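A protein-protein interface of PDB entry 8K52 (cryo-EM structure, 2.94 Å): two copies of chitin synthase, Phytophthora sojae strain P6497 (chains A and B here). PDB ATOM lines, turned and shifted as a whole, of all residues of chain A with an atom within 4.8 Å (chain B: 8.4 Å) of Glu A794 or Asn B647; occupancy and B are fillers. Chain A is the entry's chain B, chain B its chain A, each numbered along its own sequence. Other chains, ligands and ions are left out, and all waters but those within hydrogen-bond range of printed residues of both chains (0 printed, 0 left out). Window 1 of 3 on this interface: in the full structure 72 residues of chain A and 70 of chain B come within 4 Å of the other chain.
No position is printed for both chains.
Among the printed residues, merely in contact across the chains: Lys A791 with Lys B650, Lys A791 with His B651, Glu A794 with Asn B647, Ala A795 with Asn B647, Ala A795 with His B651, Arg A797 with Gly B646, Arg A797 with Asn B647, Thr A798 with Ile B642 and Thr A798 with Met B652.
The side-chain amide oxygen (OD1) of Asn B647 lies close to the backbone carbonyl oxygen (O) of Ile B643 (3.2 Å). ND2 of Asn B647 lies within hydrogen-bond range of SD of Met B652 (2.8 Å). The side-chain amide oxygen (OD1) of Asn B648 lies close to the backbone NH (N) of Lys B650 (3.3 Å). The backbone carbonyl oxygen of Asn B648 is in hydrogen-bond range of a ring nitrogen (NE2) of His B651. The side-chain carboxylate of Glu A794 is in salt-bridge range of the guanidinium group of Arg A797. The side-chain hydroxyl (OG1) of Thr A798 is in hydrogen-bond range of the backbone carbonyl oxygen (O) of Glu A794.
OD1 of Asn B647 sits at hydrogen-bond distance from OG1 of Thr A798, at 3.3 Å.
Printed residues of chain B that touch a printed residue of chain A: Ile B642, Gly B646, Asn B647, Lys B650, His B651 and Met B652. Hydrophobic or aromatic side chains of chain B within 4 Å of the printed part of chain A: Ile B642, His B651 and Met B652. Printed residues of chain A that touch a printed residue of chain B: Lys A791, Glu A794, Ala A795, Arg A797 and Thr A798. Hydrophobic or aromatic side chains of chain A that line the printed part of chain B: Ala A795. Among the printed residues, no Asp or Glu carboxylate lies within 4 Å of a Lys or Arg side-chain nitrogen of the other chain.
Glu A794 touches just one residue of chain B: Asn B647. Of chain B, only Asn B647 and His B651 come within 4 Å of Ala A795. Of the printed residues of chain B, Arg A797 touches Gly B646 (3.9 Å) and Asn B647 (3.8 Å). Of the printed residues of chain B, Thr A798 touches Ile B642 (3.9 Å), Asn B647 (3.3 Å) and Met B652 (3.5 Å). Of the printed residues of chain A, Ile B642 touches Thr A798. Gly B644 touches none of the printed residues of chain A. Asn B647 touches just these residues of chain A: Glu A794 (3.6 Å), Ala A795 (3.8 Å), Arg A797 (3.8 Å) and Thr A798 (3.3 Å). Of the printed residues of chain A, Lys B650 touches Lys A791 (3.3 Å). Of the printed residues of chain A, His B651 touches Lys A791 (3.2 Å) and Ala A795 (3.9 Å). The nearest residue of chain B that does not touch Glu A794 is His B651 (4.5 Å). The nearest printed residue of chain A that does not touch Asn B647 is Lys A791 (5.6 Å). The nearest printed residue of chain A that does not touch Ile B642 is Arg A797 (5.9 Å).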
ATOM      1  N   LYS A 790      -1.675 -18.077 -27.115  1.00  0.00           N
ATOM      2  CA  LYS A 790      -2.228 -16.776 -27.473  1.00  0.00           C
ATOM      3  C   LYS A 790      -1.127 -15.801 -27.864  1.00  0.00           C
ATOM      4  O   LYS A 790      -1.273 -15.044 -28.828  1.00  0.00           O
ATOM      5  CB  LYS A 790      -3.053 -16.220 -26.315  1.00  0.00           C
ATOM      6  CG  LYS A 790      -4.449 -16.818 -26.176  1.00  0.00           C
ATOM      7  CD  LYS A 790      -5.225 -16.779 -27.485  1.00  0.00           C
ATOM      8  CE  LYS A 790      -5.403 -18.171 -28.078  1.00  0.00           C
ATOM      9  NZ  LYS A 790      -6.514 -18.216 -29.067  1.00  0.00           N
ATOM     10  N   LYS A 791      -0.013 -15.807 -27.126  1.00  0.00           N
ATOM     11  CA  LYS A 791       1.105 -14.932 -27.454  1.00  0.00           C
ATOM     12  C   LYS A 791       1.645 -15.233 -28.843  1.00  0.00           C
ATOM     13  O   LYS A 791       1.854 -14.321 -29.648  1.00  0.00           O
ATOM     14  CB  LYS A 791       2.209 -15.081 -26.405  1.00  0.00           C
ATOM     15  CG  LYS A 791       3.620 -14.971 -26.969  1.00  0.00           C
ATOM     16  CD  LYS A 791       4.677 -15.336 -25.941  1.00  0.00           C
ATOM     17  CE  LYS A 791       6.070 -15.297 -26.552  1.00  0.00           C
ATOM     18  NZ  LYS A 791       7.123 -15.719 -25.587  1.00  0.00           N
ATOM     19  N   ASN A 792       1.867 -16.514 -29.145  1.00  0.00           N
ATOM     20  CA  ASN A 792       2.400 -16.872 -30.454  1.00  0.00           C
ATOM     21  C   ASN A 792       1.432 -16.492 -31.563  1.00  0.00           C
ATOM     22  O   ASN A 792       1.837 -15.920 -32.584  1.00  0.00           O
ATOM     23  CB  ASN A 792       2.713 -18.366 -30.505  1.00  0.00           C
ATOM     24  CG  ASN A 792       4.142 -18.673 -30.115  1.00  0.00           C
ATOM     25  OD1 ASN A 792       4.793 -17.885 -29.428  1.00  0.00           O
ATOM     26  ND2 ASN A 792       4.642 -19.822 -30.553  1.00  0.00           N
ATOM     27  N   PHE A 793       0.143 -16.785 -31.377  1.00  0.00           N
ATOM     28  CA  PHE A 793      -0.834 -16.504 -32.421  1.00  0.00           C
ATOM     29  C   PHE A 793      -0.970 -15.006 -32.657  1.00  0.00           C
ATOM     30  O   PHE A 793      -0.992 -14.549 -33.805  1.00  0.00           O
ATOM     31  CB  PHE A 793      -2.185 -17.117 -32.058  1.00  0.00           C
ATOM     32  CG  PHE A 793      -2.302 -18.568 -32.420  1.00  0.00           C
ATOM     33  CD1 PHE A 793      -1.195 -19.398 -32.382  1.00  0.00           C
ATOM     34  CD2 PHE A 793      -3.515 -19.098 -32.822  1.00  0.00           C
ATOM     35  CE1 PHE A 793      -1.297 -20.730 -32.716  1.00  0.00           C
ATOM     36  CE2 PHE A 793      -3.621 -20.428 -33.163  1.00  0.00           C
ATOM     37  CZ  PHE A 793      -2.509 -21.245 -33.112  1.00  0.00           C
ATOM     38  N   GLU A 794      -1.051 -14.222 -31.580  1.00  0.00           N
ATOM     39  CA  GLU A 794      -1.173 -12.778 -31.729  1.00  0.00           C
ATOM     40  C   GLU A 794       0.089 -12.165 -32.318  1.00  0.00           C
ATOM     41  O   GLU A 794       0.000 -11.243 -33.135  1.00  0.00           O
ATOM     42  CB  GLU A 794      -1.501 -12.136 -30.382  1.00  0.00           C
ATOM     43  CG  GLU A 794      -2.884 -12.478 -29.830  1.00  0.00           C
ATOM     44  CD  GLU A 794      -3.985 -12.442 -30.880  1.00  0.00           C
ATOM     45  OE1 GLU A 794      -4.882 -13.311 -30.825  1.00  0.00           O
ATOM     46  OE2 GLU A 794      -3.979 -11.534 -31.737  1.00  0.00           O
ATOM     47  N   ALA A 795       1.267 -12.656 -31.925  1.00  0.00           N
ATOM     48  CA  ALA A 795       2.504 -12.146 -32.502  1.00  0.00           C
ATOM     49  C   ALA A 795       2.573 -12.437 -33.992  1.00  0.00           C
ATOM     50  O   ALA A 795       2.963 -11.571 -34.781  1.00  0.00           O
ATOM     51  CB  ALA A 795       3.709 -12.748 -31.780  1.00  0.00           C
ATOM     52  N   PHE A 796       2.197 -13.651 -34.401  1.00  0.00           N
ATOM     53  CA  PHE A 796       2.191 -13.975 -35.823  1.00  0.00           C
ATOM     54  C   PHE A 796       1.182 -13.123 -36.579  1.00  0.00           C
ATOM     55  O   PHE A 796       1.471 -12.631 -37.676  1.00  0.00           O
ATOM     56  CB  PHE A 796       1.888 -15.457 -36.018  1.00  0.00           C
ATOM     57  CG  PHE A 796       1.700 -15.854 -37.453  1.00  0.00           C
ATOM     58  CD1 PHE A 796       2.793 -16.054 -38.277  1.00  0.00           C
ATOM     59  CD2 PHE A 796       0.431 -16.031 -37.975  1.00  0.00           C
ATOM     60  CE1 PHE A 796       2.624 -16.421 -39.596  1.00  0.00           C
ATOM     61  CE2 PHE A 796       0.255 -16.397 -39.293  1.00  0.00           C
ATOM     62  CZ  PHE A 796       1.353 -16.592 -40.104  1.00  0.00           C
ATOM     63  N   ARG A 797      -0.012 -12.942 -36.009  1.00  0.00           N
ATOM     64  CA  ARG A 797      -1.022 -12.109 -36.649  1.00  0.00           C
ATOM     65  C   ARG A 797      -0.510 -10.690 -36.833  1.00  0.00           C
ATOM     66  O   ARG A 797      -0.652 -10.106 -37.912  1.00  0.00           O
ATOM     67  CB  ARG A 797      -2.308 -12.128 -35.815  1.00  0.00           C
ATOM     68  CG  ARG A 797      -3.518 -11.340 -36.358  1.00  0.00           C
ATOM     69  CD  ARG A 797      -3.424  -9.821 -36.190  1.00  0.00           C
ATOM     70  NE  ARG A 797      -2.975  -9.423 -34.860  1.00  0.00           N
ATOM     71  CZ  ARG A 797      -3.760  -9.336 -33.795  1.00  0.00           C
ATOM     72  NH1 ARG A 797      -5.050  -9.622 -33.861  1.00  0.00           N
ATOM     73  NH2 ARG A 797      -3.239  -8.949 -32.634  1.00  0.00           N
ATOM     74  N   THR A 798       0.091 -10.121 -35.788  1.00  0.00           N
ATOM     75  CA  THR A 798       0.545  -8.740 -35.867  1.00  0.00           C
ATOM     76  C   THR A 798       1.724  -8.606 -36.819  1.00  0.00           C
ATOM     77  O   THR A 798       1.831  -7.613 -37.543  1.00  0.00           O
ATOM     78  CB  THR A 798       0.909  -8.226 -34.475  1.00  0.00           C
ATOM     79  OG1 THR A 798      -0.261  -8.226 -33.649  1.00  0.00           O
ATOM     80  CG2 THR A 798       1.422  -6.803 -34.564  1.00  0.00           C
ATOM     81  N   ILE B 533       6.441  -0.768 -19.724  1.00  0.00           N
ATOM     82  CA  ILE B 533       5.299  -0.496 -20.593  1.00  0.00           C
ATOM     83  C   ILE B 533       4.002  -0.896 -19.903  1.00  0.00           C
ATOM     84  O   ILE B 533       3.009  -0.164 -19.942  1.00  0.00           O
ATOM     85  CB  ILE B 533       5.466  -1.222 -21.939  1.00  0.00           C
ATOM     86  CG1 ILE B 533       6.334  -0.399 -22.890  1.00  0.00           C
ATOM     87  CG2 ILE B 533       4.115  -1.495 -22.575  1.00  0.00           C
ATOM     88  CD1 ILE B 533       6.373  -0.941 -24.294  1.00  0.00           C
ATOM     89  N   LYS B 537       1.005   1.413 -18.711  1.00  0.00           N
ATOM     90  CA  LYS B 537      -0.350   1.089 -19.125  1.00  0.00           C
ATOM     91  C   LYS B 537      -1.345   1.255 -17.993  1.00  0.00           C
ATOM     92  O   LYS B 537      -2.428   1.809 -18.212  1.00  0.00           O
ATOM     93  CB  LYS B 537      -0.412  -0.344 -19.653  1.00  0.00           C
ATOM     94  CG  LYS B 537      -1.659  -1.111 -19.241  1.00  0.00           C
ATOM     95  CD  LYS B 537      -2.598  -1.374 -20.401  1.00  0.00           C
ATOM     96  CE  LYS B 537      -3.581  -2.472 -20.034  1.00  0.00           C
ATOM     97  NZ  LYS B 537      -4.491  -2.832 -21.150  1.00  0.00           N
ATOM     98  N   MET B 639       3.185   1.702 -36.435  1.00  0.00           N
ATOM     99  CA  MET B 639       3.555   0.427 -35.834  1.00  0.00           C
ATOM    100  C   MET B 639       3.216   0.408 -34.350  1.00  0.00           C
ATOM    101  O   MET B 639       2.799  -0.624 -33.812  1.00  0.00           O
ATOM    102  CB  MET B 639       5.043   0.165 -36.065  1.00  0.00           C
ATOM    103  CG  MET B 639       5.664  -0.849 -35.131  1.00  0.00           C
ATOM    104  SD  MET B 639       7.123  -1.632 -35.843  1.00  0.00           S
ATOM    105  CE  MET B 639       7.716  -0.336 -36.925  1.00  0.00           C
ATOM    106  N   LEU B 640       3.383   1.546 -33.674  1.00  0.00           N
ATOM    107  CA  LEU B 640       3.000   1.644 -32.270  1.00  0.00           C
ATOM    108  C   LEU B 640       1.503   1.444 -32.089  1.00  0.00           C
ATOM    109  O   LEU B 640       1.082   0.710 -31.193  1.00  0.00           O
ATOM    110  CB  LEU B 640       3.429   2.996 -31.705  1.00  0.00           C
ATOM    111  CG  LEU B 640       4.913   3.206 -31.410  1.00  0.00           C
ATOM    112  CD1 LEU B 640       5.070   4.213 -30.296  1.00  0.00           C
ATOM    113  CD2 LEU B 640       5.589   1.893 -31.050  1.00  0.00           C
ATOM    114  N   ILE B 641       0.685   2.082 -32.931  1.00  0.00           N
ATOM    115  CA  ILE B 641      -0.755   1.838 -32.879  1.00  0.00           C
ATOM    116  C   ILE B 641      -1.036   0.350 -33.009  1.00  0.00           C
ATOM    117  O   ILE B 641      -1.714  -0.251 -32.161  1.00  0.00           O
ATOM    118  CB  ILE B 641      -1.495   2.620 -33.982  1.00  0.00           C
ATOM    119  CG1 ILE B 641      -1.100   4.096 -34.035  1.00  0.00           C
ATOM    120  CG2 ILE B 641      -2.994   2.472 -33.806  1.00  0.00           C
ATOM    121  CD1 ILE B 641      -1.906   4.980 -33.111  1.00  0.00           C
ATOM    122  N   ILE B 642      -0.483  -0.271 -34.053  1.00  0.00           N
ATOM    123  CA  ILE B 642      -0.816  -1.659 -34.359  1.00  0.00           C
ATOM    124  C   ILE B 642      -0.418  -2.571 -33.206  1.00  0.00           C
ATOM    125  O   ILE B 642      -1.226  -3.364 -32.710  1.00  0.00           O
ATOM    126  CB  ILE B 642      -0.152  -2.088 -35.679  1.00  0.00           C
ATOM    127  CG1 ILE B 642      -0.736  -1.290 -36.846  1.00  0.00           C
ATOM    128  CG2 ILE B 642      -0.331  -3.578 -35.907  1.00  0.00           C
ATOM    129  CD1 ILE B 642      -0.199  -1.695 -38.198  1.00  0.00           C
ATOM    130  N   ILE B 643       0.822  -2.444 -32.735  1.00  0.00           N
ATOM    131  CA  ILE B 643       1.309  -3.335 -31.688  1.00  0.00           C
ATOM    132  C   ILE B 643       0.585  -3.072 -30.374  1.00  0.00           C
ATOM    133  O   ILE B 643       0.126  -4.006 -29.706  1.00  0.00           O
ATOM    134  CB  ILE B 643       2.831  -3.194 -31.530  1.00  0.00           C
ATOM    135  CG1 ILE B 643       3.537  -3.575 -32.829  1.00  0.00           C
ATOM    136  CG2 ILE B 643       3.326  -4.067 -30.396  1.00  0.00           C
ATOM    137  CD1 ILE B 643       5.038  -3.527 -32.733  1.00  0.00           C
ATOM    138  N   GLY B 644       0.480  -1.810 -30.017  1.00  0.00           N
ATOM    139  CA  GLY B 644      -0.203  -1.468 -28.802  1.00  0.00           C
ATOM    140  C   GLY B 644      -1.566  -2.098 -28.865  1.00  0.00           C
ATOM    141  O   GLY B 644      -1.784  -3.173 -28.338  1.00  0.00           O
ATOM    142  N   LEU B 645      -2.483  -1.419 -29.527  1.00  0.00           N
ATOM    143  CA  LEU B 645      -3.844  -1.891 -29.645  1.00  0.00           C
ATOM    144  C   LEU B 645      -3.937  -3.356 -29.938  1.00  0.00           C
ATOM    145  O   LEU B 645      -4.949  -3.980 -29.672  1.00  0.00           O
ATOM    146  CB  LEU B 645      -4.545  -1.156 -30.769  1.00  0.00           C
ATOM    147  CG  LEU B 645      -5.505  -0.098 -30.269  1.00  0.00           C
ATOM    148  CD1 LEU B 645      -4.717   1.022 -29.606  1.00  0.00           C
ATOM    149  CD2 LEU B 645      -6.344   0.402 -31.430  1.00  0.00           C
ATOM    150  N   GLY B 646      -2.881  -3.912 -30.495  1.00  0.00           N
ATOM    151  CA  GLY B 646      -2.925  -5.304 -30.873  1.00  0.00           C
ATOM    152  C   GLY B 646      -2.715  -6.336 -29.798  1.00  0.00           C
ATOM    153  O   GLY B 646      -3.567  -6.590 -28.958  1.00  0.00           O
ATOM    154  N   ASN B 647      -1.547  -6.939 -29.859  1.00  0.00           N
ATOM    155  CA  ASN B 647      -1.127  -7.996 -28.952  1.00  0.00           C
ATOM    156  C   ASN B 647      -0.520  -7.431 -27.671  1.00  0.00           C
ATOM    157  O   ASN B 647      -0.273  -6.230 -27.542  1.00  0.00           O
ATOM    158  CB  ASN B 647      -0.118  -8.915 -29.636  1.00  0.00           C
ATOM    159  CG  ASN B 647       0.925  -8.151 -30.415  1.00  0.00           C
ATOM    160  OD1 ASN B 647       0.750  -6.973 -30.722  1.00  0.00           O
ATOM    161  ND2 ASN B 647       2.026  -8.818 -30.733  1.00  0.00           N
ATOM    162  N   ASN B 648      -0.287  -8.328 -26.716  1.00  0.00           N
ATOM    163  CA  ASN B 648       0.342  -7.954 -25.460  1.00  0.00           C
ATOM    164  C   ASN B 648       1.806  -7.581 -25.694  1.00  0.00           C
ATOM    165  O   ASN B 648       2.491  -8.222 -26.496  1.00  0.00           O
ATOM    166  CB  ASN B 648       0.239  -9.107 -24.460  1.00  0.00           C
ATOM    167  CG  ASN B 648       0.966  -8.828 -23.162  1.00  0.00           C
ATOM    168  OD1 ASN B 648       2.140  -9.160 -23.011  1.00  0.00           O
ATOM    169  ND2 ASN B 648       0.269  -8.214 -22.215  1.00  0.00           N
ATOM    170  N   PRO B 649       2.316  -6.556 -25.010  1.00  0.00           N
ATOM    171  CA  PRO B 649       3.697  -6.093 -25.229  1.00  0.00           C
ATOM    172  C   PRO B 649       4.727  -6.922 -24.467  1.00  0.00           C
ATOM    173  O   PRO B 649       5.466  -6.419 -23.620  1.00  0.00           O
ATOM    174  CB  PRO B 649       3.635  -4.645 -24.732  1.00  0.00           C
ATOM    175  CG  PRO B 649       2.630  -4.688 -23.645  1.00  0.00           C
ATOM    176  CD  PRO B 649       1.586  -5.676 -24.082  1.00  0.00           C
ATOM    177  N   LYS B 650       4.769  -8.204 -24.757  1.00  0.00           N
ATOM    178  CA  LYS B 650       5.803  -9.075 -24.209  1.00  0.00           C
ATOM    179  C   LYS B 650       6.505  -9.887 -25.283  1.00  0.00           C
ATOM    180  O   LYS B 650       7.724 -10.067 -25.215  1.00  0.00           O
ATOM    181  CB  LYS B 650       5.195 -10.009 -23.149  1.00  0.00           C
ATOM    182  CG  LYS B 650       5.905 -11.343 -22.993  1.00  0.00           C
ATOM    183  CD  LYS B 650       5.086 -12.470 -23.601  1.00  0.00           C
ATOM    184  CE  LYS B 650       4.146 -13.082 -22.579  1.00  0.00           C
ATOM    185  NZ  LYS B 650       3.234 -14.083 -23.198  1.00  0.00           N
ATOM    186  N   HIS B 651       5.769 -10.361 -26.285  1.00  0.00           N
ATOM    187  CA  HIS B 651       6.356 -11.109 -27.387  1.00  0.00           C
ATOM    188  C   HIS B 651       7.016 -10.206 -28.416  1.00  0.00           C
ATOM    189  O   HIS B 651       7.748 -10.704 -29.279  1.00  0.00           O
ATOM    190  CB  HIS B 651       5.282 -11.967 -28.053  1.00  0.00           C
ATOM    191  CG  HIS B 651       3.885 -11.534 -27.732  1.00  0.00           C
ATOM    192  ND1 HIS B 651       3.272 -11.830 -26.533  1.00  0.00           N
ATOM    193  CD2 HIS B 651       2.983 -10.823 -28.450  1.00  0.00           C
ATOM    194  CE1 HIS B 651       2.052 -11.325 -26.529  1.00  0.00           C
ATOM    195  NE2 HIS B 651       1.853 -10.708 -27.679  1.00  0.00           N
ATOM    196  N   MET B 652       6.774  -8.900 -28.348  1.00  0.00           N
ATOM    197  CA  MET B 652       7.430  -7.920 -29.211  1.00  0.00           C
ATOM    198  C   MET B 652       8.507  -7.141 -28.474  1.00  0.00           C
ATOM    199  O   MET B 652       8.647  -5.931 -28.666  1.00  0.00           O
ATOM    200  CB  MET B 652       6.407  -6.968 -29.821  1.00  0.00           C
ATOM    201  CG  MET B 652       4.998  -7.499 -29.865  1.00  0.00           C
ATOM    202  SD  MET B 652       4.777  -8.452 -31.375  1.00  0.00           S
ATOM    203  CE  MET B 652       4.135  -7.183 -32.456  1.00  0.00           C
ATOM    204  N   LYS B 653       9.268  -7.814 -27.609  1.00  0.00           N
ATOM    205  CA  LYS B 653      10.371  -7.148 -26.927  1.00  0.00           C
ATOM    206  C   LYS B 653      11.356  -6.561 -27.928  1.00  0.00           C
ATOM    207  O   LYS B 653      11.785  -5.410 -27.783  1.00  0.00           O
ATOM    208  CB  LYS B 653      11.077  -8.130 -25.991  1.00  0.00           C
ATOM    209  CG  LYS B 653      12.456  -7.674 -25.540  1.00  0.00           C
ATOM    210  CD  LYS B 653      13.216  -8.794 -24.848  1.00  0.00           C
ATOM    211  CE  LYS B 653      14.611  -8.343 -24.449  1.00  0.00           C
ATOM    212  NZ  LYS B 653      15.382  -9.428 -23.783  1.00  0.00           N
ATOM    213  N   THR B 655      10.847  -5.705 -31.115  1.00  0.00           N
ATOM    214  CA  THR B 655      10.263  -4.601 -31.871  1.00  0.00           C
ATOM    215  C   THR B 655      10.174  -3.338 -31.027  1.00  0.00           C
ATOM    216  O   THR B 655      10.493  -2.237 -31.501  1.00  0.00           O
ATOM    217  CB  THR B 655       8.880  -4.990 -32.388  1.00  0.00           C
ATOM    218  OG1 THR B 655       8.885  -6.369 -32.776  1.00  0.00           O
ATOM    219  CG2 THR B 655       8.508  -4.137 -33.585  1.00  0.00           C
ATOM    220  N   TYR B 656       9.735  -3.474 -29.775  1.00  0.00           N
ATOM    221  CA  TYR B 656       9.661  -2.317 -28.894  1.00  0.00           C
ATOM    222  C   TYR B 656      11.042  -1.744 -28.625  1.00  0.00           C
ATOM    223  O   TYR B 656      11.214  -0.523 -28.588  1.00  0.00           O
ATOM    224  CB  TYR B 656       8.964  -2.691 -27.589  1.00  0.00           C
ATOM    225  CG  TYR B 656       7.466  -2.516 -27.640  1.00  0.00           C
ATOM    226  CD1 TYR B 656       6.903  -1.261 -27.824  1.00  0.00           C
ATOM    227  CD2 TYR B 656       6.615  -3.601 -27.503  1.00  0.00           C
ATOM    228  CE1 TYR B 656       5.535  -1.094 -27.871  1.00  0.00           C
ATOM    229  CE2 TYR B 656       5.248  -3.442 -27.549  1.00  0.00           C
ATOM    230  CZ  TYR B 656       4.712  -2.188 -27.732  1.00  0.00           C
ATOM    231  OH  TYR B 656       3.347  -2.025 -27.779  1.00  0.00           O
ATOM    232  N   TYR B 732      -0.007   3.216 -25.703  1.00  0.00           N
ATOM    233  CA  TYR B 732      -0.460   1.916 -25.220  1.00  0.00           C
ATOM    234  C   TYR B 732      -1.491   2.067 -24.110  1.00  0.00           C
ATOM    235  O   TYR B 732      -2.390   1.230 -23.976  1.00  0.00           O
ATOM    236  CB  TYR B 732       0.726   1.074 -24.753  1.00  0.00           C
ATOM    237  CG  TYR B 732       0.317  -0.313 -24.319  1.00  0.00           C
ATOM    238  CD1 TYR B 732      -0.071  -1.265 -25.247  1.00  0.00           C
ATOM    239  CD2 TYR B 732       0.318  -0.668 -22.983  1.00  0.00           C
ATOM    240  CE1 TYR B 732      -0.454  -2.533 -24.853  1.00  0.00           C
ATOM    241  CE2 TYR B 732      -0.056  -1.933 -22.582  1.00  0.00           C
ATOM    242  CZ  TYR B 732      -0.444  -2.859 -23.515  1.00  0.00           C
ATOM    243  OH  TYR B 732      -0.822  -4.113 -23.101  1.00  0.00           O
ATOM    244  N   ASN B 736      -5.882   0.849 -24.914  1.00  0.00           N
ATOM    245  CA  ASN B 736      -6.630  -0.208 -24.247  1.00  0.00           C
ATOM    246  C   ASN B 736      -7.489   0.357 -23.122  1.00  0.00           C
ATOM    247  O   ASN B 736      -7.329  -0.013 -21.959  1.00  0.00           O
ATOM    248  CB  ASN B 736      -5.682  -1.273 -23.700  1.00  0.00           C
ATOM    249  CG  ASN B 736      -4.894  -1.966 -24.791  1.00  0.00           C
ATOM    250  OD1 ASN B 736      -3.845  -1.482 -25.216  1.00  0.00           O
ATOM    251  ND2 ASN B 736      -5.395  -3.104 -25.254  1.00  0.00           N
